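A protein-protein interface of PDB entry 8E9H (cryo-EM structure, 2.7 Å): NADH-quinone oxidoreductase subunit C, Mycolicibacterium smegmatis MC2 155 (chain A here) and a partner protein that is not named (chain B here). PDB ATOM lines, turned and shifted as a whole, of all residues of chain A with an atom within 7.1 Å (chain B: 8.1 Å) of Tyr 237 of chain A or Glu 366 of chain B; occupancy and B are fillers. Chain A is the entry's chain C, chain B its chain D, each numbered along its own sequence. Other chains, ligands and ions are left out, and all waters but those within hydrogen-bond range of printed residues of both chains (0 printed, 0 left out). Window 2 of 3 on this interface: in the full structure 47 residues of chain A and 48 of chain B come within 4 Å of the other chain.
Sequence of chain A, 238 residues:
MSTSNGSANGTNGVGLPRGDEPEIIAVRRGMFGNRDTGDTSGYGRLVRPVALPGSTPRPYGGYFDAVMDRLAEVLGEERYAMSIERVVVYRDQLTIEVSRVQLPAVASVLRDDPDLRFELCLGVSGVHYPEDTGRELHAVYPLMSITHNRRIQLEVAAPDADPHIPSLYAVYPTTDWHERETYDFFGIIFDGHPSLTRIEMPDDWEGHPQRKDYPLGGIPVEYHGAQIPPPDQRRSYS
Of chain B, only Glu 366 (3.8 Å), Arg 369 (3.8 Å) and Thr 396 (3.5 Å) come within 4 Å of Tyr 237 of chain A.
Of chain A, only Tyr 237 comes within 4 Å of Glu 366 of chain B.
Printed residues of chain B within 4 Å of Ser 236 of chain A: Arg 397.
Printed residues of chain B within 4 Å of Arg 28 of chain A: Gly 394 (3.5 Å) and Gly 395 (3.6 Å).
Printed residues of chain A within 4 Å of Gly 394 of chain B: Arg 28.
Of the printed residues of chain A, Gly 395 of chain B touches Arg 28 and Ser 238.
Of the printed residues of chain A, Thr 396 of chain B touches Tyr 237 and Ser 238.
Printed residues of chain A within 4 Å of Arg 369 of chain B: Tyr 237 (3.8 Å) and Ser 238 (3.5 Å).
Asp 39 of chain A touches none of the printed residues of chain B.
The nearest printed residue of chain B that does not touch Tyr 237 of chain A is Gly 395 of chain B (5.4 Å).
The nearest printed residue of chain A that does not touch Arg 397 of chain B is Ser 238 of chain A (4.5 Å).
ND2 of Asn 34 of chain A lies close to NH2 of Arg 235 of chain A (3.0 Å).
OD2 of Asp 36 of chain A is in salt-bridge range of NH2 of Arg 235 of chain A, 3.9 Å away.
The guanidinium group (NE) of Arg 235 of chain A sits at hydrogen-bond distance from the side-chain hydroxyl (OH) of Tyr 237 of chain A (2.8 Å).
O of Glu 366 of chain B lies close to ND2 of Asn 89 of chain B, 3.5 Å away.
NE1 of Trp 90 of chain B is in hydrogen-bond range of O of Gly 395 of chain B (3.3 Å).
N of Trp 90 of chain B sits close to O of Thr 396 of chain B, 3.2 Å away.
Of the 13 printed residues of chain A, 5 touch a printed residue of chain B.
Printed residues of chain A that touch a printed residue of chain B: Arg 28, Arg 235, Ser 236, Tyr 237 and Ser 238.
Hydrophobic or aromatic side chains of chain A that line the printed part of chain B: Tyr 237.
Along chain B the printed residues that touch a printed residue of chain A span positions 366 to 397.
The backbone carbonyl oxygen (O) of Gly 394 of chain B lies within hydrogen-bond range of the guanidinium group (NH1) of Arg 28 of chain A, at 3.5 Å.
The backbone carbonyl oxygen (O) of Ser 238 of chain A lies within hydrogen-bond range of the guanidinium group (NH1) of Arg 369 of chain B (3.5 Å).
Arg 28 of chain A touches Gly 395 of chain B.
NH2 of Arg 397 of chain B touches O of Arg 235 of chain A (3.95 Å).
Ser 236 of chain A touches Arg 397 of chain B.
Tyr 237 of chain A touches Glu 366 of chain B.
NH2 of Arg 369 of chain B touches O of Tyr 237 of chain A, at 3.8 Å.
Tyr 237 of chain A touches Thr 396 of chain B (O to OG1, 3.5 Å).
Gly 395 of chain B touches Ser 238 of chain A.
Thr 396 of chain B touches Ser 238 of chain A.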
ATOM      1  N   ARG A  28     -18.159  14.066  31.292  1.00  0.00           N
ATOM      2  CA  ARG A  28     -18.773  12.769  31.072  1.00  0.00           C
ATOM      3  C   ARG A  28     -19.652  12.412  32.260  1.00  0.00           C
ATOM      4  O   ARG A  28     -19.210  12.460  33.410  1.00  0.00           O
ATOM      5  CB  ARG A  28     -17.716  11.688  30.856  1.00  0.00           C
ATOM      6  CG  ARG A  28     -16.767  11.508  32.018  1.00  0.00           C
ATOM      7  CD  ARG A  28     -15.705  10.485  31.689  1.00  0.00           C
ATOM      8  NE  ARG A  28     -14.880  10.907  30.563  1.00  0.00           N
ATOM      9  CZ  ARG A  28     -13.925  10.168  30.017  1.00  0.00           C
ATOM     10  NH1 ARG A  28     -13.633   8.962  30.478  1.00  0.00           N
ATOM     11  NH2 ARG A  28     -13.243  10.651  28.983  1.00  0.00           N
ATOM     12  N   MET A  31     -21.086   6.285  35.111  1.00  0.00           N
ATOM     13  CA  MET A  31     -19.951   5.387  35.208  1.00  0.00           C
ATOM     14  C   MET A  31     -19.743   4.645  33.895  1.00  0.00           C
ATOM     15  O   MET A  31     -20.634   4.559  33.049  1.00  0.00           O
ATOM     16  CB  MET A  31     -20.166   4.384  36.338  1.00  0.00           C
ATOM     17  CG  MET A  31     -20.176   5.002  37.715  1.00  0.00           C
ATOM     18  SD  MET A  31     -20.525   3.796  39.003  1.00  0.00           S
ATOM     19  CE  MET A  31     -19.027   2.823  39.002  1.00  0.00           C
ATOM     20  N   PHE A  32     -18.538   4.108  33.732  1.00  0.00           N
ATOM     21  CA  PHE A  32     -18.171   3.235  32.624  1.00  0.00           C
ATOM     22  C   PHE A  32     -17.981   3.993  31.321  1.00  0.00           C
ATOM     23  O   PHE A  32     -18.006   3.382  30.249  1.00  0.00           O
ATOM     24  CB  PHE A  32     -19.216   2.134  32.428  1.00  0.00           C
ATOM     25  CG  PHE A  32     -19.593   1.439  33.701  1.00  0.00           C
ATOM     26  CD1 PHE A  32     -18.666   1.268  34.709  1.00  0.00           C
ATOM     27  CD2 PHE A  32     -20.877   0.979  33.898  1.00  0.00           C
ATOM     28  CE1 PHE A  32     -19.010   0.641  35.879  1.00  0.00           C
ATOM     29  CE2 PHE A  32     -21.223   0.349  35.068  1.00  0.00           C
ATOM     30  CZ  PHE A  32     -20.290   0.184  36.060  1.00  0.00           C
ATOM     31  N   GLY A  33     -17.804   5.308  31.379  1.00  0.00           N
ATOM     32  CA  GLY A  33     -17.478   6.080  30.199  1.00  0.00           C
ATOM     33  C   GLY A  33     -18.495   5.927  29.093  1.00  0.00           C
ATOM     34  O   GLY A  33     -18.130   5.721  27.933  1.00  0.00           O
ATOM     35  N   ASN A  34     -19.772   6.026  29.433  1.00  0.00           N
ATOM     36  CA  ASN A  34     -20.851   5.815  28.482  1.00  0.00           C
ATOM     37  C   ASN A  34     -21.482   7.155  28.131  1.00  0.00           C
ATOM     38  O   ASN A  34     -21.970   7.866  29.015  1.00  0.00           O
ATOM     39  CB  ASN A  34     -21.890   4.863  29.063  1.00  0.00           C
ATOM     40  CG  ASN A  34     -23.001   4.562  28.095  1.00  0.00           C
ATOM     41  OD1 ASN A  34     -23.019   5.065  26.973  1.00  0.00           O
ATOM     42  ND2 ASN A  34     -23.933   3.731  28.521  1.00  0.00           N
ATOM     43  N   ARG A  35     -21.470   7.494  26.842  1.00  0.00           N
ATOM     44  CA  ARG A  35     -22.055   8.755  26.396  1.00  0.00           C
ATOM     45  C   ARG A  35     -23.576   8.697  26.429  1.00  0.00           C
ATOM     46  O   ARG A  35     -24.244   9.705  26.685  1.00  0.00           O
ATOM     47  CB  ARG A  35     -21.558   9.087  24.991  1.00  0.00           C
ATOM     48  N   ASP A  36     -24.143   7.522  26.166  1.00  0.00           N
ATOM     49  CA  ASP A  36     -25.589   7.355  26.097  1.00  0.00           C
ATOM     50  C   ASP A  36     -26.193   7.223  27.490  1.00  0.00           C
ATOM     51  O   ASP A  36     -25.543   7.550  28.488  1.00  0.00           O
ATOM     52  CB  ASP A  36     -25.934   6.136  25.240  1.00  0.00           C
ATOM     53  CG  ASP A  36     -25.617   6.348  23.777  1.00  0.00           C
ATOM     54  OD1 ASP A  36     -25.686   7.504  23.315  1.00  0.00           O
ATOM     55  OD2 ASP A  36     -25.301   5.357  23.089  1.00  0.00           O
ATOM     56  N   GLY A  38     -27.067   4.598  29.322  1.00  0.00           N
ATOM     57  CA  GLY A  38     -26.621   3.551  30.222  1.00  0.00           C
ATOM     58  C   GLY A  38     -27.259   2.206  29.954  1.00  0.00           C
ATOM     59  O   GLY A  38     -28.485   2.095  29.879  1.00  0.00           O
ATOM     60  N   ASP A  39     -26.431   1.171  29.815  1.00  0.00           N
ATOM     61  CA  ASP A  39     -26.949  -0.171  29.586  1.00  0.00           C
ATOM     62  C   ASP A  39     -27.543  -0.773  30.847  1.00  0.00           C
ATOM     63  O   ASP A  39     -28.418  -1.639  30.761  1.00  0.00           O
ATOM     64  CB  ASP A  39     -25.843  -1.079  29.056  1.00  0.00           C
ATOM     65  CG  ASP A  39     -25.028  -0.423  27.969  1.00  0.00           C
ATOM     66  OD1 ASP A  39     -25.577  -0.191  26.872  1.00  0.00           O
ATOM     67  OD2 ASP A  39     -23.837  -0.140  28.207  1.00  0.00           O
ATOM     68  N   ARG A 235     -21.931   1.704  18.935  1.00  0.00           N
ATOM     69  CA  ARG A 235     -21.739   2.047  20.333  1.00  0.00           C
ATOM     70  C   ARG A 235     -20.259   2.181  20.666  1.00  0.00           C
ATOM     71  O   ARG A 235     -19.397   1.575  20.029  1.00  0.00           O
ATOM     72  CB  ARG A 235     -22.374   0.978  21.211  1.00  0.00           C
ATOM     73  CG  ARG A 235     -22.751   1.454  22.575  1.00  0.00           C
ATOM     74  CD  ARG A 235     -23.867   0.620  23.151  1.00  0.00           C
ATOM     75  NE  ARG A 235     -24.246   1.107  24.467  1.00  0.00           N
ATOM     76  CZ  ARG A 235     -24.768   2.302  24.698  1.00  0.00           C
ATOM     77  NH1 ARG A 235     -25.102   3.113  23.709  1.00  0.00           N
ATOM     78  NH2 ARG A 235     -24.966   2.689  25.951  1.00  0.00           N
ATOM     79  N   SER A 236     -19.971   2.991  21.681  1.00  0.00           N
ATOM     80  CA  SER A 236     -18.615   3.147  22.183  1.00  0.00           C
ATOM     81  C   SER A 236     -18.683   3.540  23.648  1.00  0.00           C
ATOM     82  O   SER A 236     -19.692   4.063  24.123  1.00  0.00           O
ATOM     83  CB  SER A 236     -17.836   4.199  21.394  1.00  0.00           C
ATOM     84  OG  SER A 236     -18.386   5.486  21.603  1.00  0.00           O
ATOM     85  N   TYR A 237     -17.588   3.295  24.360  1.00  0.00           N
ATOM     86  CA  TYR A 237     -17.509   3.560  25.790  1.00  0.00           C
ATOM     87  C   TYR A 237     -16.247   4.335  26.124  1.00  0.00           C
ATOM     88  O   TYR A 237     -15.530   4.013  27.073  1.00  0.00           O
ATOM     89  CB  TYR A 237     -17.568   2.260  26.583  1.00  0.00           C
ATOM     90  CG  TYR A 237     -18.886   1.553  26.442  1.00  0.00           C
ATOM     91  CD1 TYR A 237     -19.936   1.827  27.299  1.00  0.00           C
ATOM     92  CD2 TYR A 237     -19.085   0.621  25.439  1.00  0.00           C
ATOM     93  CE1 TYR A 237     -21.144   1.186  27.166  1.00  0.00           C
ATOM     94  CE2 TYR A 237     -20.287  -0.024  25.299  1.00  0.00           C
ATOM     95  CZ  TYR A 237     -21.313   0.261  26.165  1.00  0.00           C
ATOM     96  OH  TYR A 237     -22.517  -0.382  26.026  1.00  0.00           O
ATOM     97  N   SER A 238     -15.959   5.371  25.347  1.00  0.00           N
ATOM     98  CA  SER A 238     -14.797   6.210  25.601  1.00  0.00           C
ATOM     99  C   SER A 238     -14.952   6.955  26.922  1.00  0.00           C
ATOM    100  O   SER A 238     -14.833   6.367  27.996  1.00  0.00           O
ATOM    101  CB  SER A 238     -14.593   7.203  24.456  1.00  0.00           C
ATOM    102  N   ARG B  88     -11.211   4.117  17.263  1.00  0.00           N
ATOM    103  CA  ARG B  88     -10.697   2.810  17.632  1.00  0.00           C
ATOM    104  C   ARG B  88      -9.910   2.940  18.924  1.00  0.00           C
ATOM    105  O   ARG B  88      -9.276   3.962  19.184  1.00  0.00           O
ATOM    106  CB  ARG B  88      -9.802   2.227  16.537  1.00  0.00           C
ATOM    107  CG  ARG B  88     -10.470   2.141  15.192  1.00  0.00           C
ATOM    108  CD  ARG B  88     -11.601   1.146  15.205  1.00  0.00           C
ATOM    109  NE  ARG B  88     -12.251   1.060  13.906  1.00  0.00           N
ATOM    110  CZ  ARG B  88     -13.309   0.308  13.647  1.00  0.00           C
ATOM    111  NH1 ARG B  88     -13.858  -0.455  14.578  1.00  0.00           N
ATOM    112  NH2 ARG B  88     -13.827   0.318  12.425  1.00  0.00           N
ATOM    113  N   ASN B  89      -9.947   1.890  19.732  1.00  0.00           N
ATOM    114  CA  ASN B  89      -9.270   1.947  21.014  1.00  0.00           C
ATOM    115  C   ASN B  89      -7.761   2.005  20.816  1.00  0.00           C
ATOM    116  O   ASN B  89      -7.247   1.911  19.702  1.00  0.00           O
ATOM    117  CB  ASN B  89      -9.643   0.742  21.875  1.00  0.00           C
ATOM    118  CG  ASN B  89      -9.182  -0.571  21.280  1.00  0.00           C
ATOM    119  OD1 ASN B  89      -8.251  -0.616  20.483  1.00  0.00           O
ATOM    120  ND2 ASN B  89      -9.838  -1.653  21.668  1.00  0.00           N
ATOM    121  N   TRP B  90      -7.052   2.176  21.923  1.00  0.00           N
ATOM    122  CA  TRP B  90      -5.608   2.020  21.896  1.00  0.00           C
ATOM    123  C   TRP B  90      -5.278   0.568  21.580  1.00  0.00           C
ATOM    124  O   TRP B  90      -6.060  -0.338  21.875  1.00  0.00           O
ATOM    125  CB  TRP B  90      -5.001   2.422  23.237  1.00  0.00           C
ATOM    126  CG  TRP B  90      -5.545   3.697  23.805  1.00  0.00           C
ATOM    127  CD1 TRP B  90      -6.604   3.827  24.648  1.00  0.00           C
ATOM    128  CD2 TRP B  90      -5.042   5.017  23.591  1.00  0.00           C
ATOM    129  NE1 TRP B  90      -6.801   5.145  24.963  1.00  0.00           N
ATOM    130  CE2 TRP B  90      -5.853   5.897  24.328  1.00  0.00           C
ATOM    131  CE3 TRP B  90      -3.988   5.541  22.845  1.00  0.00           C
ATOM    132  CZ2 TRP B  90      -5.644   7.265  24.337  1.00  0.00           C
ATOM    133  CZ3 TRP B  90      -3.783   6.899  22.858  1.00  0.00           C
ATOM    134  CH2 TRP B  90      -4.604   7.747  23.597  1.00  0.00           C
ATOM    135  N   THR B  91      -4.121   0.348  20.964  1.00  0.00           N
ATOM    136  CA  THR B  91      -3.723  -0.978  20.502  1.00  0.00           C
ATOM    137  C   THR B  91      -4.483  -1.368  19.243  1.00  0.00           C
ATOM    138  O   THR B  91      -4.188  -2.397  18.630  1.00  0.00           O
ATOM    139  CB  THR B  91      -3.945  -2.043  21.578  1.00  0.00           C
ATOM    140  OG1 THR B  91      -5.336  -2.372  21.644  1.00  0.00           O
ATOM    141  CG2 THR B  91      -3.472  -1.554  22.935  1.00  0.00           C
ATOM    142  N   GLN B  92      -5.467  -0.559  18.851  1.00  0.00           N
ATOM    143  CA  GLN B  92      -5.991  -0.644  17.495  1.00  0.00           C
ATOM    144  C   GLN B  92      -5.432   0.487  16.651  1.00  0.00           C
ATOM    145  O   GLN B  92      -5.253   0.342  15.438  1.00  0.00           O
ATOM    146  CB  GLN B  92      -7.515  -0.596  17.505  1.00  0.00           C
ATOM    147  CG  GLN B  92      -8.170  -1.940  17.709  1.00  0.00           C
ATOM    148  CD  GLN B  92      -9.674  -1.840  17.781  1.00  0.00           C
ATOM    149  OE1 GLN B  92     -10.221  -0.802  18.144  1.00  0.00           O
ATOM    150  NE2 GLN B  92     -10.353  -2.917  17.424  1.00  0.00           N
ATOM    151  N   TRP B 328      -1.199  -6.209  27.507  1.00  0.00           N
ATOM    152  CA  TRP B 328      -2.012  -6.882  26.509  1.00  0.00           C
ATOM    153  C   TRP B 328      -2.188  -8.335  26.930  1.00  0.00           C
ATOM    154  O   TRP B 328      -1.188  -9.051  27.080  1.00  0.00           O
ATOM    155  CB  TRP B 328      -1.349  -6.795  25.140  1.00  0.00           C
ATOM    156  CG  TRP B 328      -2.174  -7.325  24.024  1.00  0.00           C
ATOM    157  CD1 TRP B 328      -1.878  -8.384  23.225  1.00  0.00           C
ATOM    158  CD2 TRP B 328      -3.432  -6.822  23.575  1.00  0.00           C
ATOM    159  NE1 TRP B 328      -2.874  -8.573  22.303  1.00  0.00           N
ATOM    160  CE2 TRP B 328      -3.841  -7.626  22.498  1.00  0.00           C
ATOM    161  CE3 TRP B 328      -4.256  -5.773  23.982  1.00  0.00           C
ATOM    162  CZ2 TRP B 328      -5.036  -7.412  21.822  1.00  0.00           C
ATOM    163  CZ3 TRP B 328      -5.439  -5.563  23.308  1.00  0.00           C
ATOM    164  CH2 TRP B 328      -5.818  -6.378  22.242  1.00  0.00           C
ATOM    165  N   HIS B 359     -10.135  -9.566  32.718  1.00  0.00           N
ATOM    166  CA  HIS B 359      -9.072  -8.733  32.177  1.00  0.00           C
ATOM    167  C   HIS B 359      -8.870  -8.990  30.696  1.00  0.00           C
ATOM    168  O   HIS B 359      -8.730  -8.048  29.910  1.00  0.00           O
ATOM    169  CB  HIS B 359      -7.783  -8.972  32.952  1.00  0.00           C
ATOM    170  CG  HIS B 359      -7.737  -8.249  34.258  1.00  0.00           C
ATOM    171  ND1 HIS B 359      -8.514  -8.612  35.335  1.00  0.00           N
ATOM    172  CD2 HIS B 359      -7.016  -7.176  34.657  1.00  0.00           C
ATOM    173  CE1 HIS B 359      -8.273  -7.796  36.343  1.00  0.00           C
ATOM    174  NE2 HIS B 359      -7.367  -6.916  35.958  1.00  0.00           N
ATOM    175  N   HIS B 360      -8.854 -10.256  30.287  1.00  0.00           N
ATOM    176  CA  HIS B 360      -8.741 -10.554  28.867  1.00  0.00           C
ATOM    177  C   HIS B 360      -9.869  -9.892  28.093  1.00  0.00           C
ATOM    178  O   HIS B 360      -9.639  -9.150  27.132  1.00  0.00           O
ATOM    179  CB  HIS B 360      -8.758 -12.062  28.648  1.00  0.00           C
ATOM    180  CG  HIS B 360      -8.795 -12.455  27.209  1.00  0.00           C
ATOM    181  ND1 HIS B 360      -7.660 -12.547  26.435  1.00  0.00           N
ATOM    182  CD2 HIS B 360      -9.832 -12.753  26.393  1.00  0.00           C
ATOM    183  CE1 HIS B 360      -7.994 -12.904  25.209  1.00  0.00           C
ATOM    184  NE2 HIS B 360      -9.307 -13.031  25.156  1.00  0.00           N
ATOM    185  N   PHE B 361     -11.105 -10.125  28.530  1.00  0.00           N
ATOM    186  CA  PHE B 361     -12.267  -9.591  27.837  1.00  0.00           C
ATOM    187  C   PHE B 361     -12.167  -8.081  27.691  1.00  0.00           C
ATOM    188  O   PHE B 361     -12.341  -7.535  26.598  1.00  0.00           O
ATOM    189  CB  PHE B 361     -13.527  -9.989  28.605  1.00  0.00           C
ATOM    190  CG  PHE B 361     -14.804  -9.712  27.874  1.00  0.00           C
ATOM    191  CD1 PHE B 361     -15.231  -8.420  27.656  1.00  0.00           C
ATOM    192  CD2 PHE B 361     -15.584 -10.751  27.418  1.00  0.00           C
ATOM    193  CE1 PHE B 361     -16.404  -8.171  26.995  1.00  0.00           C
ATOM    194  CE2 PHE B 361     -16.760 -10.505  26.756  1.00  0.00           C
ATOM    195  CZ  PHE B 361     -17.169  -9.213  26.542  1.00  0.00           C
ATOM    196  N   LYS B 362     -11.881  -7.384  28.788  1.00  0.00           N
ATOM    197  CA  LYS B 362     -11.917  -5.929  28.752  1.00  0.00           C
ATOM    198  C   LYS B 362     -10.745  -5.354  27.971  1.00  0.00           C
ATOM    199  O   LYS B 362     -10.933  -4.473  27.127  1.00  0.00           O
ATOM    200  CB  LYS B 362     -11.942  -5.373  30.172  1.00  0.00           C
ATOM    201  CG  LYS B 362     -13.215  -5.689  30.935  1.00  0.00           C
ATOM    202  CD  LYS B 362     -14.462  -5.156  30.251  1.00  0.00           C
ATOM    203  CE  LYS B 362     -14.393  -3.663  30.029  1.00  0.00           C
ATOM    204  NZ  LYS B 362     -15.712  -3.128  29.622  1.00  0.00           N
ATOM    205  N   LEU B 363      -9.527  -5.827  28.232  1.00  0.00           N
ATOM    206  CA  LEU B 363      -8.375  -5.253  27.552  1.00  0.00           C
ATOM    207  C   LEU B 363      -8.399  -5.559  26.065  1.00  0.00           C
ATOM    208  O   LEU B 363      -7.878  -4.778  25.263  1.00  0.00           O
ATOM    209  CB  LEU B 363      -7.086  -5.771  28.178  1.00  0.00           C
ATOM    210  CG  LEU B 363      -6.913  -5.436  29.657  1.00  0.00           C
ATOM    211  CD1 LEU B 363      -5.699  -6.133  30.217  1.00  0.00           C
ATOM    212  CD2 LEU B 363      -6.799  -3.943  29.856  1.00  0.00           C
ATOM    213  N   VAL B 364      -8.983  -6.689  25.676  1.00  0.00           N
ATOM    214  CA  VAL B 364      -9.103  -7.002  24.259  1.00  0.00           C
ATOM    215  C   VAL B 364     -10.196  -6.167  23.609  1.00  0.00           C
ATOM    216  O   VAL B 364     -10.033  -5.673  22.488  1.00  0.00           O
ATOM    217  CB  VAL B 364      -9.360  -8.507  24.085  1.00  0.00           C
ATOM    218  CG1 VAL B 364      -9.602  -8.847  22.648  1.00  0.00           C
ATOM    219  CG2 VAL B 364      -8.172  -9.293  24.588  1.00  0.00           C
ATOM    220  N   THR B 365     -11.325  -6.002  24.288  1.00  0.00           N
ATOM    221  CA  THR B 365     -12.497  -5.425  23.646  1.00  0.00           C
ATOM    222  C   THR B 365     -12.443  -3.909  23.582  1.00  0.00           C
ATOM    223  O   THR B 365     -12.368  -3.334  22.493  1.00  0.00           O
ATOM    224  CB  THR B 365     -13.755  -5.852  24.390  1.00  0.00           C
ATOM    225  OG1 THR B 365     -13.598  -5.594  25.789  1.00  0.00           O
ATOM    226  CG2 THR B 365     -14.022  -7.311  24.171  1.00  0.00           C
ATOM    227  N   GLU B 366     -12.472  -3.250  24.739  1.00  0.00           N
ATOM    228  CA  GLU B 366     -12.430  -1.794  24.740  1.00  0.00           C
ATOM    229  C   GLU B 366     -11.026  -1.283  25.004  1.00  0.00           C
ATOM    230  O   GLU B 366     -10.719  -0.129  24.691  1.00  0.00           O
ATOM    231  CB  GLU B 366     -13.404  -1.234  25.773  1.00  0.00           C
ATOM    232  CG  GLU B 366     -12.993  -1.452  27.210  1.00  0.00           C
ATOM    233  CD  GLU B 366     -13.989  -0.859  28.181  1.00  0.00           C
ATOM    234  OE1 GLU B 366     -15.043  -0.372  27.724  1.00  0.00           O
ATOM    235  OE2 GLU B 366     -13.720  -0.877  29.399  1.00  0.00           O
ATOM    236  N   GLY B 367     -10.168  -2.113  25.575  1.00  0.00           N
ATOM    237  CA  GLY B 367      -8.777  -1.760  25.768  1.00  0.00           C
ATOM    238  C   GLY B 367      -8.573  -0.886  26.986  1.00  0.00           C
ATOM    239  O   GLY B 367      -9.504  -0.525  27.710  1.00  0.00           O
ATOM    240  N   ILE B 368      -7.302  -0.551  27.204  1.00  0.00           N
ATOM    241  CA  ILE B 368      -6.947   0.326  28.305  1.00  0.00           C
ATOM    242  C   ILE B 368      -7.563   1.697  28.083  1.00  0.00           C
ATOM    243  O   ILE B 368      -7.835   2.107  26.950  1.00  0.00           O
ATOM    244  CB  ILE B 368      -5.419   0.430  28.430  1.00  0.00           C
ATOM    245  CG1 ILE B 368      -4.812   0.931  27.120  1.00  0.00           C
ATOM    246  CG2 ILE B 368      -4.837  -0.917  28.769  1.00  0.00           C
ATOM    247  CD1 ILE B 368      -3.392   1.376  27.251  1.00  0.00           C
ATOM    248  N   ARG B 369      -7.788   2.415  29.177  1.00  0.00           N
ATOM    249  CA  ARG B 369      -8.189   3.813  29.124  1.00  0.00           C
ATOM    250  C   ARG B 369      -7.045   4.653  29.667  1.00  0.00           C
ATOM    251  O   ARG B 369      -6.612   4.461  30.807  1.00  0.00           O
ATOM    252  CB  ARG B 369      -9.474   4.060  29.914  1.00  0.00           C
ATOM    253  CG  ARG B 369      -9.463   3.514  31.321  1.00  0.00           C
ATOM    254  CD  ARG B 369     -10.811   3.700  31.990  1.00  0.00           C
ATOM    255  NE  ARG B 369     -11.866   2.936  31.331  1.00  0.00           N
ATOM    256  CZ  ARG B 369     -12.872   3.458  30.643  1.00  0.00           C
ATOM    257  NH1 ARG B 369     -12.996   4.763  30.467  1.00  0.00           N
ATOM    258  NH2 ARG B 369     -13.783   2.645  30.114  1.00  0.00           N
ATOM    259  N   GLY B 394      -9.130  10.737  28.671  1.00  0.00           N
ATOM    260  CA  GLY B 394      -9.450   9.776  29.698  1.00  0.00           C
ATOM    261  C   GLY B 394     -10.195   8.557  29.213  1.00  0.00           C
ATOM    262  O   GLY B 394     -10.463   7.658  30.017  1.00  0.00           O
ATOM    263  N   GLY B 395     -10.528   8.489  27.928  1.00  0.00           N
ATOM    264  CA  GLY B 395     -11.323   7.402  27.405  1.00  0.00           C
ATOM    265  C   GLY B 395     -10.477   6.275  26.859  1.00  0.00           C
ATOM    266  O   GLY B 395      -9.249   6.300  26.886  1.00  0.00           O
ATOM    267  N   THR B 396     -11.167   5.262  26.344  1.00  0.00           N
ATOM    268  CA  THR B 396     -10.503   4.100  25.781  1.00  0.00           C
ATOM    269  C   THR B 396     -10.020   4.328  24.358  1.00  0.00           C
ATOM    270  O   THR B 396      -9.374   3.440  23.795  1.00  0.00           O
ATOM    271  CB  THR B 396     -11.443   2.899  25.812  1.00  0.00           C
ATOM    272  OG1 THR B 396     -12.669   3.234  25.152  1.00  0.00           O
ATOM    273  CG2 THR B 396     -11.740   2.504  27.243  1.00  0.00           C
ATOM    274  N   ARG B 397     -10.320   5.479  23.766  1.00  0.00           N
ATOM    275  CA  ARG B 397      -9.890   5.807  22.421  1.00  0.00           C
ATOM    276  C   ARG B 397      -9.024   7.057  22.440  1.00  0.00           C
ATOM    277  O   ARG B 397      -9.229   7.943  23.274  1.00  0.00           O
ATOM    278  CB  ARG B 397     -11.093   6.043  21.503  1.00  0.00           C
ATOM    279  CG  ARG B 397     -12.065   4.891  21.452  1.00  0.00           C
ATOM    280  CD  ARG B 397     -13.285   5.255  20.644  1.00  0.00           C
ATOM    281  NE  ARG B 397     -14.061   4.081  20.274  1.00  0.00           N
ATOM    282  CZ  ARG B 397     -15.165   4.113  19.543  1.00  0.00           C
ATOM    283  NH1 ARG B 397     -15.666   5.254  19.100  1.00  0.00           N
ATOM    284  NH2 ARG B 397     -15.784   2.974  19.253  1.00  0.00           N
